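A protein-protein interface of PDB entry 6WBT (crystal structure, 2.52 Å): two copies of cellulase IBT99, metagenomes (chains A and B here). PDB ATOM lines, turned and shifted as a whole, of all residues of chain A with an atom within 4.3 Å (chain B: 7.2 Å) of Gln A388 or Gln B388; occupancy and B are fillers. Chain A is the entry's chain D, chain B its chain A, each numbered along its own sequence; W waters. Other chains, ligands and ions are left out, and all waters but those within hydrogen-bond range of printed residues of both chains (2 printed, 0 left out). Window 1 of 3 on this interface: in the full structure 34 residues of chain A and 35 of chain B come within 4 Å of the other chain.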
ATOM      1  N   GLY A 384       5.601  17.736  23.683  1.00  0.00           N
ATOM      2  CA  GLY A 384       5.551  16.458  22.990  1.00  0.00           C
ATOM      3  C   GLY A 384       4.944  15.352  23.830  1.00  0.00           C
ATOM      4  O   GLY A 384       4.189  14.518  23.323  1.00  0.00           O
ATOM      5  N   LEU A 385       5.263  15.327  25.126  1.00  0.00           N
ATOM      6  CA  LEU A 385       4.685  14.315  26.005  1.00  0.00           C
ATOM      7  C   LEU A 385       3.192  14.543  26.202  1.00  0.00           C
ATOM      8  O   LEU A 385       2.409  13.586  26.220  1.00  0.00           O
ATOM      9  CB  LEU A 385       5.408  14.309  27.351  1.00  0.00           C
ATOM     10  CG  LEU A 385       6.857  13.818  27.352  1.00  0.00           C
ATOM     11  CD1 LEU A 385       7.441  13.900  28.752  1.00  0.00           C
ATOM     12  CD2 LEU A 385       6.942  12.398  26.816  1.00  0.00           C
ATOM     13  N   ILE A 386       2.777  15.803  26.348  1.00  0.00           N
ATOM     14  CA  ILE A 386       1.361  16.099  26.542  1.00  0.00           C
ATOM     15  C   ILE A 386       0.583  15.873  25.252  1.00  0.00           C
ATOM     16  O   ILE A 386      -0.533  15.341  25.271  1.00  0.00           O
ATOM     17  CB  ILE A 386       1.183  17.531  27.077  1.00  0.00           C
ATOM     18  CG1 ILE A 386       1.722  17.634  28.505  1.00  0.00           C
ATOM     19  CG2 ILE A 386      -0.278  17.945  27.034  1.00  0.00           C
ATOM     20  CD1 ILE A 386       1.640  19.027  29.088  1.00  0.00           C
ATOM     21  N   GLU A 387       1.158  16.266  24.108  1.00  0.00           N
ATOM     22  CA  GLU A 387       0.487  16.045  22.830  1.00  0.00           C
ATOM     23  C   GLU A 387       0.233  14.565  22.579  1.00  0.00           C
ATOM     24  O   GLU A 387      -0.780  14.203  21.970  1.00  0.00           O
ATOM     25  CB  GLU A 387       1.314  16.638  21.686  1.00  0.00           C
ATOM     26  CG  GLU A 387       1.258  18.157  21.578  1.00  0.00           C
ATOM     27  CD  GLU A 387      -0.016  18.659  20.925  1.00  0.00           C
ATOM     28  OE1 GLU A 387      -0.861  17.825  20.535  1.00  0.00           O
ATOM     29  OE2 GLU A 387      -0.169  19.891  20.795  1.00  0.00           O
ATOM     30  N   GLN A 388       1.135  13.699  23.042  1.00  0.00           N
ATOM     31  CA  GLN A 388       0.945  12.263  22.866  1.00  0.00           C
ATOM     32  C   GLN A 388      -0.177  11.745  23.758  1.00  0.00           C
ATOM     33  O   GLN A 388      -1.052  11.001  23.303  1.00  0.00           O
ATOM     34  CB  GLN A 388       2.251  11.522  23.155  1.00  0.00           C
ATOM     35  CG  GLN A 388       2.144  10.013  23.021  1.00  0.00           C
ATOM     36  CD  GLN A 388       3.443   9.304  23.341  1.00  0.00           C
ATOM     37  OE1 GLN A 388       4.401   9.918  23.812  1.00  0.00           O
ATOM     38  NE2 GLN A 388       3.483   8.002  23.086  1.00  0.00           N
ATOM     39  N   GLN A 389      -0.166  12.130  25.037  1.00  0.00           N
ATOM     40  CA  GLN A 389      -1.195  11.657  25.957  1.00  0.00           C
ATOM     41  C   GLN A 389      -2.547  12.286  25.645  1.00  0.00           C
ATOM     42  O   GLN A 389      -3.589  11.639  25.804  1.00  0.00           O
ATOM     43  CB  GLN A 389      -0.783  11.949  27.400  1.00  0.00           C
ATOM     44  CG  GLN A 389      -1.680  11.312  28.452  1.00  0.00           C
ATOM     45  CD  GLN A 389      -1.552   9.799  28.496  1.00  0.00           C
ATOM     46  OE1 GLN A 389      -0.567   9.232  28.023  1.00  0.00           O
ATOM     47  NE2 GLN A 389      -2.553   9.137  29.066  1.00  0.00           N
ATOM     48  N   ASP A 390      -2.554  13.547  25.203  1.00  0.00           N
ATOM     49  CA  ASP A 390      -3.814  14.191  24.850  1.00  0.00           C
ATOM     50  C   ASP A 390      -4.450  13.526  23.635  1.00  0.00           C
ATOM     51  O   ASP A 390      -5.663  13.293  23.612  1.00  0.00           O
ATOM     52  CB  ASP A 390      -3.591  15.681  24.593  1.00  0.00           C
ATOM     53  CG  ASP A 390      -4.885  16.426  24.337  1.00  0.00           C
ATOM     54  OD1 ASP A 390      -5.694  16.552  25.279  1.00  0.00           O
ATOM     55  OD2 ASP A 390      -5.095  16.880  23.192  1.00  0.00           O
ATOM     56  N   ALA A 391      -3.644  13.214  22.618  1.00  0.00           N
ATOM     57  CA  ALA A 391      -4.148  12.444  21.488  1.00  0.00           C
ATOM     58  C   ALA A 391      -4.549  11.037  21.909  1.00  0.00           C
ATOM     59  O   ALA A 391      -5.504  10.475  21.361  1.00  0.00           O
ATOM     60  CB  ALA A 391      -3.098  12.389  20.377  1.00  0.00           C
ATOM     61  N   CYS A 392      -3.840  10.459  22.883  1.00  0.00           N
ATOM     62  CA  CYS A 392      -4.210   9.139  23.386  1.00  0.00           C
ATOM     63  C   CYS A 392      -5.572   9.175  24.066  1.00  0.00           C
ATOM     64  O   CYS A 392      -6.434   8.327  23.808  1.00  0.00           O
ATOM     65  CB  CYS A 392      -3.139   8.628  24.351  1.00  0.00           C
ATOM     66  SG  CYS A 392      -3.616   7.166  25.306  1.00  0.00           S
ATOM     67  N   MET A 414      -1.172   4.632  21.091  1.00  0.00           N
ATOM     68  CA  MET A 414      -0.590   5.937  21.386  1.00  0.00           C
ATOM     69  C   MET A 414       0.043   5.997  22.775  1.00  0.00           C
ATOM     70  O   MET A 414       1.004   6.737  22.993  1.00  0.00           O
ATOM     71  CB  MET A 414      -1.654   7.028  21.258  1.00  0.00           C
ATOM     72  CG  MET A 414      -1.105   8.443  21.302  1.00  0.00           C
ATOM     73  SD  MET A 414      -0.107   8.901  19.694  1.00  0.00           S
ATOM     74  CE  MET A 414      -1.565   8.772  18.408  1.00  0.00           C
ATOM     75  N   ARG A 416       2.186   5.520  26.036  1.00  0.00           N
ATOM     76  CA  ARG A 416       3.616   5.246  26.143  1.00  0.00           C
ATOM     77  C   ARG A 416       3.882   3.886  26.773  1.00  0.00           C
ATOM     78  O   ARG A 416       4.809   3.177  26.363  1.00  0.00           O
ATOM     79  CB  ARG A 416       4.308   6.344  26.951  1.00  0.00           C
ATOM     80  CG  ARG A 416       4.222   7.730  26.338  1.00  0.00           C
ATOM     81  CD  ARG A 416       5.131   8.709  27.064  1.00  0.00           C
ATOM     82  NE  ARG A 416       6.537   8.330  26.956  1.00  0.00           N
ATOM     83  CZ  ARG A 416       7.341   8.718  25.971  1.00  0.00           C
ATOM     84  NH1 ARG A 416       6.880   9.501  25.006  1.00  0.00           N
ATOM     85  NH2 ARG A 416       8.607   8.324  25.952  1.00  0.00           N
ATOM     86  N   LEU B 199       6.312  12.918   8.310  1.00  0.00           N
ATOM     87  CA  LEU B 199       7.738  13.198   8.364  1.00  0.00           C
ATOM     88  C   LEU B 199       8.496  12.191   7.503  1.00  0.00           C
ATOM     89  O   LEU B 199       7.926  11.237   6.971  1.00  0.00           O
ATOM     90  CB  LEU B 199       8.243  13.160   9.809  1.00  0.00           C
ATOM     91  CG  LEU B 199       7.540  14.085  10.805  1.00  0.00           C
ATOM     92  CD1 LEU B 199       8.169  13.964  12.184  1.00  0.00           C
ATOM     93  CD2 LEU B 199       7.573  15.528  10.323  1.00  0.00           C
ATOM     94  N   TYR B 202       8.116   8.480   8.030  1.00  0.00           N
ATOM     95  CA  TYR B 202       7.128   8.661   9.086  1.00  0.00           C
ATOM     96  C   TYR B 202       5.846   9.249   8.508  1.00  0.00           C
ATOM     97  O   TYR B 202       5.231  10.130   9.117  1.00  0.00           O
ATOM     98  CB  TYR B 202       7.691   9.568  10.181  1.00  0.00           C
ATOM     99  CG  TYR B 202       7.160   9.298  11.572  1.00  0.00           C
ATOM    100  CD1 TYR B 202       7.622   8.218  12.311  1.00  0.00           C
ATOM    101  CD2 TYR B 202       6.213  10.134  12.151  1.00  0.00           C
ATOM    102  CE1 TYR B 202       7.148   7.969  13.581  1.00  0.00           C
ATOM    103  CE2 TYR B 202       5.734   9.893  13.424  1.00  0.00           C
ATOM    104  CZ  TYR B 202       6.206   8.809  14.133  1.00  0.00           C
ATOM    105  OH  TYR B 202       5.733   8.562  15.401  1.00  0.00           O
ATOM    106  N   LYS B 383      -1.764  13.167  14.054  1.00  0.00           N
ATOM    107  CA  LYS B 383      -1.168  14.348  14.668  1.00  0.00           C
ATOM    108  C   LYS B 383      -0.324  13.964  15.877  1.00  0.00           C
ATOM    109  O   LYS B 383       0.824  14.405  16.011  1.00  0.00           O
ATOM    110  CB  LYS B 383      -2.259  15.341  15.069  1.00  0.00           C
ATOM    111  CG  LYS B 383      -1.772  16.474  15.959  1.00  0.00           C
ATOM    112  CD  LYS B 383      -2.933  17.312  16.472  1.00  0.00           C
ATOM    113  CE  LYS B 383      -2.471  18.340  17.495  1.00  0.00           C
ATOM    114  NZ  LYS B 383      -1.494  19.306  16.922  1.00  0.00           N
ATOM    115  N   GLY B 384      -0.877  13.135  16.766  1.00  0.00           N
ATOM    116  CA  GLY B 384      -0.159  12.765  17.973  1.00  0.00           C
ATOM    117  C   GLY B 384       1.115  11.989  17.701  1.00  0.00           C
ATOM    118  O   GLY B 384       2.095  12.120  18.439  1.00  0.00           O
ATOM    119  N   LEU B 385       1.122  11.174  16.644  1.00  0.00           N
ATOM    120  CA  LEU B 385       2.334  10.445  16.281  1.00  0.00           C
ATOM    121  C   LEU B 385       3.403  11.387  15.744  1.00  0.00           C
ATOM    122  O   LEU B 385       4.586  11.247  16.075  1.00  0.00           O
ATOM    123  CB  LEU B 385       2.005   9.360  15.255  1.00  0.00           C
ATOM    124  CG  LEU B 385       1.288   8.116  15.779  1.00  0.00           C
ATOM    125  CD1 LEU B 385       0.875   7.213  14.629  1.00  0.00           C
ATOM    126  CD2 LEU B 385       2.179   7.364  16.755  1.00  0.00           C
ATOM    127  N   ILE B 386       3.007  12.356  14.913  1.00  0.00           N
ATOM    128  CA  ILE B 386       3.974  13.303  14.370  1.00  0.00           C
ATOM    129  C   ILE B 386       4.431  14.284  15.444  1.00  0.00           C
ATOM    130  O   ILE B 386       5.597  14.697  15.460  1.00  0.00           O
ATOM    131  CB  ILE B 386       3.379  14.028  13.148  1.00  0.00           C
ATOM    132  CG1 ILE B 386       3.083  13.025  12.030  1.00  0.00           C
ATOM    133  CG2 ILE B 386       4.322  15.109  12.642  1.00  0.00           C
ATOM    134  CD1 ILE B 386       2.410  13.638  10.821  1.00  0.00           C
ATOM    135  N   GLU B 387       3.537  14.661  16.363  1.00  0.00           N
ATOM    136  CA  GLU B 387       3.918  15.583  17.431  1.00  0.00           C
ATOM    137  C   GLU B 387       5.004  14.987  18.318  1.00  0.00           C
ATOM    138  O   GLU B 387       5.896  15.705  18.786  1.00  0.00           O
ATOM    139  CB  GLU B 387       2.694  15.959  18.270  1.00  0.00           C
ATOM    140  CG  GLU B 387       1.737  16.939  17.602  1.00  0.00           C
ATOM    141  CD  GLU B 387       2.270  18.360  17.560  1.00  0.00           C
ATOM    142  OE1 GLU B 387       3.358  18.613  18.118  1.00  0.00           O
ATOM    143  OE2 GLU B 387       1.593  19.229  16.970  1.00  0.00           O
ATOM    144  N   GLN B 388       4.950  13.676  18.559  1.00  0.00           N
ATOM    145  CA  GLN B 388       5.963  13.037  19.392  1.00  0.00           C
ATOM    146  C   GLN B 388       7.316  13.016  18.691  1.00  0.00           C
ATOM    147  O   GLN B 388       8.342  13.363  19.287  1.00  0.00           O
ATOM    148  CB  GLN B 388       5.524  11.621  19.762  1.00  0.00           C
ATOM    149  CG  GLN B 388       6.531  10.867  20.615  1.00  0.00           C
ATOM    150  CD  GLN B 388       6.052   9.482  20.997  1.00  0.00           C
ATOM    151  OE1 GLN B 388       4.966   9.059  20.604  1.00  0.00           O
ATOM    152  NE2 GLN B 388       6.863   8.768  21.768  1.00  0.00           N
ATOM    153  N   GLN B 389       7.336  12.610  17.418  1.00  0.00           N
ATOM    154  CA  GLN B 389       8.596  12.546  16.684  1.00  0.00           C
ATOM    155  C   GLN B 389       9.155  13.937  16.415  1.00  0.00           C
ATOM    156  O   GLN B 389      10.372  14.145  16.492  1.00  0.00           O
ATOM    157  CB  GLN B 389       8.401  11.784  15.374  1.00  0.00           C
ATOM    158  CG  GLN B 389       8.969  10.375  15.387  1.00  0.00           C
ATOM    159  CD  GLN B 389      10.484  10.355  15.350  1.00  0.00           C
ATOM    160  OE1 GLN B 389      11.139  10.192  16.379  1.00  0.00           O
ATOM    161  NE2 GLN B 389      11.049  10.517  14.160  1.00  0.00           N
ATOM    162  N   ASP B 390       8.288  14.900  16.094  1.00  0.00           N
ATOM    163  CA  ASP B 390       8.759  16.258  15.840  1.00  0.00           C
ATOM    164  C   ASP B 390       9.383  16.863  17.091  1.00  0.00           C
ATOM    165  O   ASP B 390      10.381  17.588  17.009  1.00  0.00           O
ATOM    166  CB  ASP B 390       7.612  17.131  15.334  1.00  0.00           C
ATOM    167  CG  ASP B 390       8.095  18.425  14.714  1.00  0.00           C
ATOM    168  OD1 ASP B 390       8.712  18.368  13.630  1.00  0.00           O
ATOM    169  OD2 ASP B 390       7.860  19.498  15.308  1.00  0.00           O
ATOM    170  N   ALA B 391       8.806  16.576  18.261  1.00  0.00           N
ATOM    171  CA  ALA B 391       9.434  16.992  19.509  1.00  0.00           C
ATOM    172  C   ALA B 391      10.736  16.237  19.739  1.00  0.00           C
ATOM    173  O   ALA B 391      11.727  16.821  20.192  1.00  0.00           O
ATOM    174  CB  ALA B 391       8.474  16.781  20.678  1.00  0.00           C
ATOM    175  N   CYS B 392      10.752  14.939  19.425  1.00  0.00           N
ATOM    176  CA  CYS B 392      11.973  14.152  19.557  1.00  0.00           C
ATOM    177  C   CYS B 392      13.076  14.692  18.655  1.00  0.00           C
ATOM    178  O   CYS B 392      14.197  14.949  19.108  1.00  0.00           O
ATOM    179  CB  CYS B 392      11.683  12.686  19.234  1.00  0.00           C
ATOM    180  SG  CYS B 392      13.151  11.671  18.983  1.00  0.00           S
ATOM    181  N   GLU B 393      12.773  14.869  17.367  1.00  0.00           N
ATOM    182  CA  GLU B 393      13.762  15.418  16.446  1.00  0.00           C
ATOM    183  C   GLU B 393      14.085  16.870  16.770  1.00  0.00           C
ATOM    184  O   GLU B 393      15.218  17.314  16.555  1.00  0.00           O
ATOM    185  CB  GLU B 393      13.265  15.289  15.006  1.00  0.00           C
ATOM    186  CG  GLU B 393      13.019  13.856  14.564  1.00  0.00           C
ATOM    187  CD  GLU B 393      12.427  13.768  13.172  1.00  0.00           C
ATOM    188  OE1 GLU B 393      12.093  14.826  12.599  1.00  0.00           O
ATOM    189  OE2 GLU B 393      12.294  12.640  12.652  1.00  0.00           O
ATOM    190  N   GLY B 394      13.110  17.621  17.288  1.00  0.00           N
ATOM    191  CA  GLY B 394      13.376  19.000  17.663  1.00  0.00           C
ATOM    192  C   GLY B 394      14.308  19.111  18.855  1.00  0.00           C
ATOM    193  O   GLY B 394      15.201  19.964  18.877  1.00  0.00           O
ATOM    194  N   LEU B 395      14.116  18.254  19.860  1.00  0.00           N
ATOM    195  CA  LEU B 395      15.005  18.260  21.018  1.00  0.00           C
ATOM    196  C   LEU B 395      16.411  17.808  20.648  1.00  0.00           C
ATOM    197  O   LEU B 395      17.385  18.243  21.274  1.00  0.00           O
ATOM    198  CB  LEU B 395      14.436  17.371  22.123  1.00  0.00           C
ATOM    199  CG  LEU B 395      13.160  17.858  22.813  1.00  0.00           C
ATOM    200  CD1 LEU B 395      12.525  16.732  23.611  1.00  0.00           C
ATOM    201  CD2 LEU B 395      13.453  19.052  23.706  1.00  0.00           C
ATOM    202  N   ALA B 411      15.549  13.812  23.993  1.00  0.00           N
ATOM    203  CA  ALA B 411      15.298  13.319  22.644  1.00  0.00           C
ATOM    204  C   ALA B 411      15.194  11.799  22.622  1.00  0.00           C
ATOM    205  O   ALA B 411      14.349  11.238  21.914  1.00  0.00           O
ATOM    206  CB  ALA B 411      16.396  13.797  21.695  1.00  0.00           C
ATOM    207  N   THR B 413      14.437   9.850  25.301  1.00  0.00           N
ATOM    208  CA  THR B 413      13.268   9.452  26.079  1.00  0.00           C
ATOM    209  C   THR B 413      11.983   9.586  25.268  1.00  0.00           C
ATOM    210  O   THR B 413      11.064   8.773  25.421  1.00  0.00           O
ATOM    211  CB  THR B 413      13.182  10.292  27.357  1.00  0.00           C
ATOM    212  OG1 THR B 413      14.366  10.096  28.143  1.00  0.00           O
ATOM    213  CG2 THR B 413      11.963   9.903  28.183  1.00  0.00           C
ATOM    214  N   MET B 414      11.911  10.583  24.393  1.00  0.00           N
ATOM    215  CA  MET B 414      10.705  10.860  23.619  1.00  0.00           C
ATOM    216  C   MET B 414      10.418   9.797  22.557  1.00  0.00           C
ATOM    217  O   MET B 414       9.260   9.535  22.231  1.00  0.00           O
ATOM    218  CB  MET B 414      10.822  12.234  22.951  1.00  0.00           C
ATOM    219  CG  MET B 414       9.585  12.669  22.184  1.00  0.00           C
ATOM    220  SD  MET B 414       8.089  13.106  23.349  1.00  0.00           S
ATOM    221  CE  MET B 414       8.899  14.599  24.304  1.00  0.00           C
ATOM    222  N   ASN B 415      11.477   9.188  22.027  1.00  0.00           N
ATOM    223  CA  ASN B 415      11.332   8.275  20.900  1.00  0.00           C
ATOM    224  C   ASN B 415      10.508   7.053  21.286  1.00  0.00           C
ATOM    225  O   ASN B 415      10.584   6.558  22.414  1.00  0.00           O
ATOM    226  CB  ASN B 415      12.709   7.844  20.392  1.00  0.00           C
ATOM    227  CG  ASN B 415      12.653   7.244  19.002  1.00  0.00           C
ATOM    228  OD1 ASN B 415      12.360   6.061  18.833  1.00  0.00           O
ATOM    229  ND2 ASN B 415      12.938   8.061  17.994  1.00  0.00           N
ATOM    230  N   ARG B 416       9.711   6.565  20.330  1.00  0.00           N
ATOM    231  CA  ARG B 416       8.841   5.422  20.596  1.00  0.00           C
ATOM    232  C   ARG B 416       9.631   4.126  20.721  1.00  0.00           C
ATOM    233  O   ARG B 416       9.198   3.206  21.427  1.00  0.00           O
ATOM    234  CB  ARG B 416       7.788   5.291  19.495  1.00  0.00           C
ATOM    235  CG  ARG B 416       6.895   6.511  19.333  1.00  0.00           C
ATOM    236  CD  ARG B 416       5.776   6.249  18.339  1.00  0.00           C
ATOM    237  NE  ARG B 416       4.875   5.194  18.797  1.00  0.00           N
ATOM    238  CZ  ARG B 416       3.810   5.403  19.563  1.00  0.00           C
ATOM    239  NH1 ARG B 416       3.508   6.631  19.962  1.00  0.00           N
ATOM    240  NH2 ARG B 416       3.046   4.384  19.932  1.00  0.00           N
ATOM    241  N   THR B 417      10.776   4.027  20.042  1.00  0.00           N
ATOM    242  CA  THR B 417      11.584   2.813  20.126  1.00  0.00           C
ATOM    243  C   THR B 417      12.121   2.603  21.537  1.00  0.00           C
ATOM    244  O   THR B 417      12.175   1.467  22.025  1.00  0.00           O
ATOM    245  CB  THR B 417      12.732   2.877  19.117  1.00  0.00           C
ATOM    246  OG1 THR B 417      12.201   2.924  17.787  1.00  0.00           O
ATOM    247  CG2 THR B 417      13.642   1.665  19.251  1.00  0.00           C
ATOM    248  N   ILE B 418      12.507   3.682  22.209  1.00  0.00           N
ATOM    249  CA  ILE B 418      13.048   3.601  23.563  1.00  0.00           C
ATOM    250  C   ILE B 418      11.898   3.381  24.538  1.00  0.00           C
ATOM    251  O   ILE B 418      10.962   4.193  24.585  1.00  0.00           O
ATOM    252  CB  ILE B 418      13.849   4.863  23.918  1.00  0.00           C
ATOM    253  CG1 ILE B 418      14.757   5.259  22.752  1.00  0.00           C
ATOM    254  CG2 ILE B 418      14.671   4.631  25.174  1.00  0.00           C
ATOM    255  CD1 ILE B 418      15.754   4.197  22.361  1.00  0.00           C
HETATM  256  O   HOH W   1      11.069   6.006  26.429  1.00  0.00           O
HETATM  257  O   HOH W   2      -1.385  21.647  19.235  1.00  0.00           O
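The side-chain amide nitrogen (NE2) of Gln B388 lies within hydrogen-bond range of the backbone carbonyl oxygen (O) of Met B414 (2.6 Å). O of Met A414 lies within hydrogen-bond range of NE2 of Gln A388. The side-chain amide oxygen (OE1) of Gln B388 lies within hydrogen-bond range of the guanidinium group (NH1) of Arg B416, 2.9 Å away. NH1 of Arg A416 lies within hydrogen-bond range of OE1 of Gln A388, at 2.8 Å. NZ of Lys B383 is in salt-bridge range of OE2 of Glu B387. OH of Tyr B202 is in hydrogen-bond range of O of Leu B385, at 3.0 Å.
NE2 of Gln A388 sits at hydrogen-bond distance from OE1 of Gln B388 (3.1 Å). The guanidinium group (NH1) of Arg A416 sits close to the side-chain amide nitrogen (NE2) of Gln B388. The backbone carbonyl oxygen (O) of Thr B413 sits at hydrogen-bond distance from the guanidinium group (NH2) of Arg A416, at 2.6 Å. NH1 of Arg B416 sits close to NE2 of Gln A388 (3.4 Å). The side-chain amino group of Lys B383 is in salt-bridge range of the side-chain carboxylate of Glu A387.
Water W1 lies within hydrogen-bond range of O of Ile B418, O of Thr B413 and NH2 of Arg A416. Water W2 bridges OE2 of Glu A387 (2.6 Å) and NZ of Lys B383 (3.3 Å).
Ala B391 touches Gly A384. Gly A384 touches Met B414 (C to SD, 3.9 Å). Met B414 touches Leu A385. CB of Glu B387 touches CB of Glu A387, at 3.7 Å. Ala A391 touches Gly B384. Met A414 touches Gly B384 (SD to C, 3.9 Å). Leu B385 touches Met A414. Met A414 touches Arg B416 (O to NH1, 3.9 Å). Arg A416 touches Met B414.
Along chain A the printed residues that touch a printed residue of chain B span positions 384 to 416. Hydrophobic or aromatic side chains of chain B that line the printed part of chain A: Leu B385, Ala B391 and Met B414. Among the printed residues, 14 pairs touch across the chains. Among the printed residues, Asp or Glu carboxylates within 4 Å of a Lys or Arg side-chain nitrogen of the other chain: Glu A387 with Lys B383 (3.96 Å).
Of the printed residues of chain B, Glu A387 touches Lys B383 (3.5 Å) and Glu B387 (3.7 Å). Of chain B, only Gln B388 (3.1 Å) and Arg B416 (3.4 Å) come within 4 Å of Gln A388. Gln A389 touches none of the printed residues of chain B. Printed residues of chain B within 4 Å of Ala A391: Gly B384. Of the printed residues of chain B, Arg A416 touches Gln B388, Thr B413 and Met B414. Ile B386 touches none of the printed residues of chain A. Of the printed residues of chain A, Glu B387 touches Glu A387 (3.7 Å). Printed residues of chain A within 4 Å of Gln B388: Gln A388 (3.1 Å) and Arg A416 (3.3 Å). Of the printed residues of chain A, Met B414 touches Gly A384 (3.9 Å), Leu A385 (3.7 Å) and Arg A416 (3.7 Å). The nearest printed residue of chain A that does not touch Gln B388 is Gly A384 (4.6 Å). The nearest printed residue of chain A that does not touch Arg B416 is Arg A416 (6.0 Å).
Gly A384 touches Ala B391, and with the chains exchanged Ala A391 touches Gly B384. Leu A385 touches Met B414, and with the chains exchanged Met A414 touches Leu B385. Gln B388 touches its own counterpart, Gln A388. Met A414 touches Arg B416, and with the chains exchanged Arg A416 touches Met B414.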
